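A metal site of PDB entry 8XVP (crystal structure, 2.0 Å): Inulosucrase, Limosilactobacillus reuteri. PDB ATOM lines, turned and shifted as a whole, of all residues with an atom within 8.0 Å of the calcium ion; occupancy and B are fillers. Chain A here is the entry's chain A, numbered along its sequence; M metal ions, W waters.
The calcium ion is bound by the backbone carbonyl oxygen (O) of Trp 486 (2.3 Å), the side-chain amide oxygen (OD1) of Asn 488 (2.3 Å), the side-chain carboxylate (OD1) of Asp 418 (2.3 Å), water W1 (2.3 Å), the side-chain amide oxygen (OE1) of Gln 449 (2.3 Å), the side-chain carboxylate (OD1) of Asp 520 (2.5 Å) and the side-chain carboxylate (OD2) of Asp 520 (2.6 Å).
Water W1 lies within hydrogen-bond range of O of Asn 419 (2.7 Å), OG of Ser 442 (2.7 Å) and OE1 of Gln 405 (3.2 Å).
The nearest printed residue that does not touch the calcium ion is Asn 419 (4.4 Å).
The backbone carbonyl oxygen of Ser 519 lies within hydrogen-bond range of the backbone NH of Asn 488 (3.4 Å). O of Asn 488 sits at hydrogen-bond distance from N of Thr 443 (2.8 Å). OD2 of Asp 418 is in hydrogen-bond range of NE2 of Gln 405 (3.1 Å). The indole nitrogen (NE1) of Trp 410 lies within hydrogen-bond range of the backbone carbonyl oxygen (O) of Asp 418 (2.9 Å). The side-chain amide nitrogen of Gln 449 sits close to the side-chain amide nitrogen of Gln 405 (3.4 Å). The backbone carbonyl oxygen (O) of Asp 520 is in hydrogen-bond range of the side-chain amide nitrogen (ND2) of Asn 419.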
ATOM      1  N   GLN A 405       7.332 -18.313  24.708  1.00  0.00           N
ATOM      2  CA  GLN A 405       7.718 -17.283  25.679  1.00  0.00           C
ATOM      3  C   GLN A 405       6.517 -16.717  26.434  1.00  0.00           C
ATOM      4  O   GLN A 405       5.450 -16.446  25.853  1.00  0.00           O
ATOM      5  CB  GLN A 405       8.486 -16.168  24.967  1.00  0.00           C
ATOM      6  CG  GLN A 405       9.009 -15.061  25.880  1.00  0.00           C
ATOM      7  CD  GLN A 405       9.508 -13.858  25.086  1.00  0.00           C
ATOM      8  OE1 GLN A 405       8.757 -13.254  24.332  1.00  0.00           O
ATOM      9  NE2 GLN A 405      10.782 -13.493  25.289  1.00  0.00           N
ATOM     10  N   TRP A 410       9.434 -12.327  29.119  1.00  0.00           N
ATOM     11  CA  TRP A 410       9.701 -11.146  28.314  1.00  0.00           C
ATOM     12  C   TRP A 410      10.052  -9.978  29.211  1.00  0.00           C
ATOM     13  O   TRP A 410      11.032  -9.257  28.975  1.00  0.00           O
ATOM     14  CB  TRP A 410       8.462 -10.780  27.492  1.00  0.00           C
ATOM     15  CG  TRP A 410       8.558  -9.453  26.788  1.00  0.00           C
ATOM     16  CD1 TRP A 410       9.260  -9.164  25.659  1.00  0.00           C
ATOM     17  CD2 TRP A 410       7.919  -8.238  27.187  1.00  0.00           C
ATOM     18  NE1 TRP A 410       9.076  -7.841  25.306  1.00  0.00           N
ATOM     19  CE2 TRP A 410       8.269  -7.254  26.238  1.00  0.00           C
ATOM     20  CE3 TRP A 410       7.057  -7.904  28.234  1.00  0.00           C
ATOM     21  CZ2 TRP A 410       7.789  -5.945  26.310  1.00  0.00           C
ATOM     22  CZ3 TRP A 410       6.590  -6.596  28.305  1.00  0.00           C
ATOM     23  CH2 TRP A 410       6.961  -5.633  27.353  1.00  0.00           C
ATOM     24  N   ALA A 417      14.232  -3.971  23.264  1.00  0.00           N
ATOM     25  CA  ALA A 417      14.619  -4.602  22.019  1.00  0.00           C
ATOM     26  C   ALA A 417      13.911  -5.943  21.790  1.00  0.00           C
ATOM     27  O   ALA A 417      14.104  -6.540  20.748  1.00  0.00           O
ATOM     28  CB  ALA A 417      16.128  -4.790  21.993  1.00  0.00           C
ATOM     29  N   ASP A 418      13.100  -6.425  22.735  1.00  0.00           N
ATOM     30  CA  ASP A 418      12.441  -7.699  22.566  1.00  0.00           C
ATOM     31  C   ASP A 418      11.000  -7.486  22.254  1.00  0.00           C
ATOM     32  O   ASP A 418      10.322  -6.714  22.920  1.00  0.00           O
ATOM     33  CB  ASP A 418      12.561  -8.593  23.828  1.00  0.00           C
ATOM     34  CG  ASP A 418      12.334 -10.030  23.535  1.00  0.00           C
ATOM     35  OD1 ASP A 418      12.445 -10.429  22.342  1.00  0.00           O
ATOM     36  OD2 ASP A 418      12.059 -10.796  24.500  1.00  0.00           O
ATOM     37  N   ASN A 419      10.505  -8.189  21.241  1.00  0.00           N
ATOM     38  CA  ASN A 419       9.099  -8.160  20.924  1.00  0.00           C
ATOM     39  C   ASN A 419       8.316  -9.054  21.880  1.00  0.00           C
ATOM     40  O   ASN A 419       8.857  -9.960  22.473  1.00  0.00           O
ATOM     41  CB  ASN A 419       8.879  -8.567  19.462  1.00  0.00           C
ATOM     42  CG  ASN A 419       7.514  -8.156  18.953  1.00  0.00           C
ATOM     43  OD1 ASN A 419       6.832  -7.270  19.521  1.00  0.00           O
ATOM     44  ND2 ASN A 419       7.100  -8.794  17.892  1.00  0.00           N
ATOM     45  N   ILE A 420       7.049  -8.741  22.081  1.00  0.00           N
ATOM     46  CA  ILE A 420       6.189  -9.608  22.865  1.00  0.00           C
ATOM     47  C   ILE A 420       5.036 -10.001  21.963  1.00  0.00           C
ATOM     48  O   ILE A 420       4.406  -9.135  21.366  1.00  0.00           O
ATOM     49  CB  ILE A 420       5.679  -8.961  24.191  1.00  0.00           C
ATOM     50  CG1 ILE A 420       4.612  -9.882  24.819  1.00  0.00           C
ATOM     51  CG2 ILE A 420       5.116  -7.554  23.997  1.00  0.00           C
ATOM     52  CD1 ILE A 420       4.231  -9.546  26.223  1.00  0.00           C
ATOM     53  N   ALA A 421       4.773 -11.297  21.860  1.00  0.00           N
ATOM     54  CA  ALA A 421       3.755 -11.841  20.986  1.00  0.00           C
ATOM     55  C   ALA A 421       3.120 -13.067  21.571  1.00  0.00           C
ATOM     56  O   ALA A 421       3.809 -14.045  21.900  1.00  0.00           O
ATOM     57  CB  ALA A 421       4.345 -12.152  19.627  1.00  0.00           C
ATOM     58  N   ALA A 441       3.590 -16.452  18.344  1.00  0.00           N
ATOM     59  CA  ALA A 441       4.287 -16.362  19.604  1.00  0.00           C
ATOM     60  C   ALA A 441       5.776 -16.167  19.365  1.00  0.00           C
ATOM     61  O   ALA A 441       6.192 -15.827  18.230  1.00  0.00           O
ATOM     62  CB  ALA A 441       3.993 -17.611  20.438  1.00  0.00           C
ATOM     63  N   SER A 442       6.569 -16.298  20.429  1.00  0.00           N
ATOM     64  CA  SER A 442       8.031 -16.347  20.352  1.00  0.00           C
ATOM     65  C   SER A 442       8.443 -17.654  21.042  1.00  0.00           C
ATOM     66  O   SER A 442       7.676 -18.156  21.910  1.00  0.00           O
ATOM     67  CB  SER A 442       8.675 -15.182  21.109  1.00  0.00           C
ATOM     68  OG  SER A 442       8.208 -13.912  20.705  1.00  0.00           O
ATOM     69  N   THR A 443       9.595 -18.208  20.680  1.00  0.00           N
ATOM     70  CA  THR A 443      10.022 -19.507  21.286  1.00  0.00           C
ATOM     71  C   THR A 443      10.309 -19.327  22.771  1.00  0.00           C
ATOM     72  O   THR A 443      10.646 -18.238  23.209  1.00  0.00           O
ATOM     73  CB  THR A 443      11.313 -20.073  20.679  1.00  0.00           C
ATOM     74  OG1 THR A 443      12.375 -19.118  20.801  1.00  0.00           O
ATOM     75  CG2 THR A 443      11.126 -20.479  19.242  1.00  0.00           C
ATOM     76  N   TYR A 448      15.714 -20.845  22.919  1.00  0.00           N
ATOM     77  CA  TYR A 448      15.381 -19.466  23.258  1.00  0.00           C
ATOM     78  C   TYR A 448      16.216 -18.476  22.511  1.00  0.00           C
ATOM     79  O   TYR A 448      17.322 -18.783  22.112  1.00  0.00           O
ATOM     80  CB  TYR A 448      15.550 -19.233  24.759  1.00  0.00           C
ATOM     81  CG  TYR A 448      14.730 -18.107  25.346  1.00  0.00           C
ATOM     82  CD1 TYR A 448      13.396 -17.900  24.986  1.00  0.00           C
ATOM     83  CD2 TYR A 448      15.289 -17.260  26.319  1.00  0.00           C
ATOM     84  CE1 TYR A 448      12.645 -16.871  25.537  1.00  0.00           C
ATOM     85  CE2 TYR A 448      14.552 -16.231  26.868  1.00  0.00           C
ATOM     86  CZ  TYR A 448      13.230 -16.039  26.497  1.00  0.00           C
ATOM     87  OH  TYR A 448      12.504 -15.045  27.076  1.00  0.00           O
ATOM     88  N   GLN A 449      15.676 -17.271  22.377  1.00  0.00           N
ATOM     89  CA  GLN A 449      16.451 -16.142  21.886  1.00  0.00           C
ATOM     90  C   GLN A 449      17.704 -15.990  22.715  1.00  0.00           C
ATOM     91  O   GLN A 449      17.709 -16.289  23.910  1.00  0.00           O
ATOM     92  CB  GLN A 449      15.666 -14.847  22.030  1.00  0.00           C
ATOM     93  CG  GLN A 449      15.256 -14.543  23.482  1.00  0.00           C
ATOM     94  CD  GLN A 449      14.165 -13.512  23.571  1.00  0.00           C
ATOM     95  OE1 GLN A 449      13.427 -13.284  22.603  1.00  0.00           O
ATOM     96  NE2 GLN A 449      14.064 -12.882  24.728  1.00  0.00           N
ATOM     97  N   GLY A 450      18.748 -15.459  22.083  1.00  0.00           N
ATOM     98  CA  GLY A 450      19.939 -15.043  22.815  1.00  0.00           C
ATOM     99  C   GLY A 450      21.096 -14.827  21.859  1.00  0.00           C
ATOM    100  O   GLY A 450      21.008 -15.122  20.652  1.00  0.00           O
ATOM    101  N   ARG A 483      19.303  -7.382  17.010  1.00  0.00           N
ATOM    102  CA  ARG A 483      18.142  -8.030  16.429  1.00  0.00           C
ATOM    103  C   ARG A 483      18.318  -9.545  16.430  1.00  0.00           C
ATOM    104  O   ARG A 483      17.483 -10.245  16.844  1.00  0.00           O
ATOM    105  CB  ARG A 483      17.903  -7.505  15.016  1.00  0.00           C
ATOM    106  CG  ARG A 483      17.473  -6.056  14.971  1.00  0.00           C
ATOM    107  CD  ARG A 483      17.153  -5.620  13.566  1.00  0.00           C
ATOM    108  NE  ARG A 483      16.556  -4.300  13.535  1.00  0.00           N
ATOM    109  CZ  ARG A 483      15.370  -4.022  13.015  1.00  0.00           C
ATOM    110  NH1 ARG A 483      14.644  -4.970  12.492  1.00  0.00           N
ATOM    111  NH2 ARG A 483      14.921  -2.802  13.037  1.00  0.00           N
ATOM    112  N   ALA A 484      19.448 -10.013  15.955  1.00  0.00           N
ATOM    113  CA  ALA A 484      19.752 -11.449  15.930  1.00  0.00           C
ATOM    114  C   ALA A 484      19.690 -12.073  17.328  1.00  0.00           C
ATOM    115  O   ALA A 484      19.257 -13.197  17.497  1.00  0.00           O
ATOM    116  CB  ALA A 484      21.127 -11.678  15.319  1.00  0.00           C
ATOM    117  N   THR A 485      20.147 -11.307  18.313  1.00  0.00           N
ATOM    118  CA  THR A 485      20.134 -11.697  19.729  1.00  0.00           C
ATOM    119  C   THR A 485      18.745 -11.822  20.343  1.00  0.00           C
ATOM    120  O   THR A 485      18.541 -12.591  21.297  1.00  0.00           O
ATOM    121  CB  THR A 485      20.975 -10.684  20.545  1.00  0.00           C
ATOM    122  OG1 THR A 485      22.342 -10.773  20.110  1.00  0.00           O
ATOM    123  CG2 THR A 485      20.907 -10.944  22.075  1.00  0.00           C
ATOM    124  N   TRP A 486      17.798 -11.063  19.805  1.00  0.00           N
ATOM    125  CA  TRP A 486      16.467 -11.032  20.339  1.00  0.00           C
ATOM    126  C   TRP A 486      15.449 -11.753  19.465  1.00  0.00           C
ATOM    127  O   TRP A 486      14.328 -11.968  19.898  1.00  0.00           O
ATOM    128  CB  TRP A 486      16.055  -9.579  20.575  1.00  0.00           C
ATOM    129  CG  TRP A 486      16.832  -8.913  21.696  1.00  0.00           C
ATOM    130  CD1 TRP A 486      17.830  -7.980  21.566  1.00  0.00           C
ATOM    131  CD2 TRP A 486      16.651  -9.129  23.099  1.00  0.00           C
ATOM    132  NE1 TRP A 486      18.293  -7.629  22.818  1.00  0.00           N
ATOM    133  CE2 TRP A 486      17.591  -8.326  23.779  1.00  0.00           C
ATOM    134  CE3 TRP A 486      15.810  -9.963  23.858  1.00  0.00           C
ATOM    135  CZ2 TRP A 486      17.677  -8.281  25.173  1.00  0.00           C
ATOM    136  CZ3 TRP A 486      15.907  -9.919  25.230  1.00  0.00           C
ATOM    137  CH2 TRP A 486      16.837  -9.082  25.889  1.00  0.00           C
ATOM    138  N   ALA A 487      15.832 -12.146  18.267  1.00  0.00           N
ATOM    139  CA  ALA A 487      14.878 -12.747  17.314  1.00  0.00           C
ATOM    140  C   ALA A 487      14.523 -14.183  17.642  1.00  0.00           C
ATOM    141  O   ALA A 487      15.407 -15.035  17.688  1.00  0.00           O
ATOM    142  CB  ALA A 487      15.447 -12.663  15.905  1.00  0.00           C
ATOM    143  N   ASN A 488      13.246 -14.475  17.800  1.00  0.00           N
ATOM    144  CA  ASN A 488      12.780 -15.838  17.999  1.00  0.00           C
ATOM    145  C   ASN A 488      11.276 -16.019  17.793  1.00  0.00           C
ATOM    146  O   ASN A 488      10.574 -16.699  18.580  1.00  0.00           O
ATOM    147  CB  ASN A 488      13.169 -16.347  19.407  1.00  0.00           C
ATOM    148  CG  ASN A 488      12.443 -15.617  20.489  1.00  0.00           C
ATOM    149  OD1 ASN A 488      12.060 -14.454  20.321  1.00  0.00           O
ATOM    150  ND2 ASN A 488      12.247 -16.288  21.649  1.00  0.00           N
ATOM    151  N   ALA A 489      10.801 -15.453  16.680  1.00  0.00           N
ATOM    152  CA  ALA A 489       9.411 -15.556  16.318  1.00  0.00           C
ATOM    153  C   ALA A 489       9.050 -17.017  16.140  1.00  0.00           C
ATOM    154  O   ALA A 489       9.884 -17.843  15.696  1.00  0.00           O
ATOM    155  CB  ALA A 489       9.143 -14.809  15.028  1.00  0.00           C
ATOM    156  N   SER A 519      13.957 -13.367  12.671  1.00  0.00           N
ATOM    157  CA  SER A 519      12.885 -12.419  12.812  1.00  0.00           C
ATOM    158  C   SER A 519      12.247 -12.533  14.154  1.00  0.00           C
ATOM    159  O   SER A 519      12.182 -13.582  14.674  1.00  0.00           O
ATOM    160  CB  SER A 519      11.813 -12.644  11.795  1.00  0.00           C
ATOM    161  OG  SER A 519      10.844 -11.712  11.951  1.00  0.00           O
ATOM    162  N   ASP A 520      11.758 -11.422  14.666  1.00  0.00           N
ATOM    163  CA  ASP A 520      11.071 -11.412  15.937  1.00  0.00           C
ATOM    164  C   ASP A 520       9.570 -11.120  15.814  1.00  0.00           C
ATOM    165  O   ASP A 520       8.916 -10.861  16.790  1.00  0.00           O
ATOM    166  CB  ASP A 520      11.716 -10.501  16.943  1.00  0.00           C
ATOM    167  CG  ASP A 520      11.610 -11.031  18.353  1.00  0.00           C
ATOM    168  OD1 ASP A 520      11.435 -12.215  18.494  1.00  0.00           O
ATOM    169  OD2 ASP A 520      11.707 -10.251  19.276  1.00  0.00           O
ATOM    170  N   GLU A 521       9.065 -11.185  14.581  1.00  0.00           N
ATOM    171  CA  GLU A 521       7.667 -10.977  14.314  1.00  0.00           C
ATOM    172  C   GLU A 521       7.103 -11.582  13.032  1.00  0.00           C
ATOM    173  O   GLU A 521       7.379 -11.106  11.973  1.00  0.00           O
ATOM    174  CB  GLU A 521       7.292  -9.501  14.379  1.00  0.00           C
ATOM    175  CG  GLU A 521       5.823  -9.245  14.496  1.00  0.00           C
ATOM    176  CD  GLU A 521       5.548  -7.795  14.648  1.00  0.00           C
ATOM    177  OE1 GLU A 521       5.457  -7.091  13.657  1.00  0.00           O
ATOM    178  OE2 GLU A 521       5.427  -7.371  15.780  1.00  0.00           O
HETATM  179 CA    CA M   1      12.268 -12.214  20.864  1.00  0.00          CA
HETATM  180  O   HOH W   1      10.043 -12.179  21.586  1.00  0.00           O
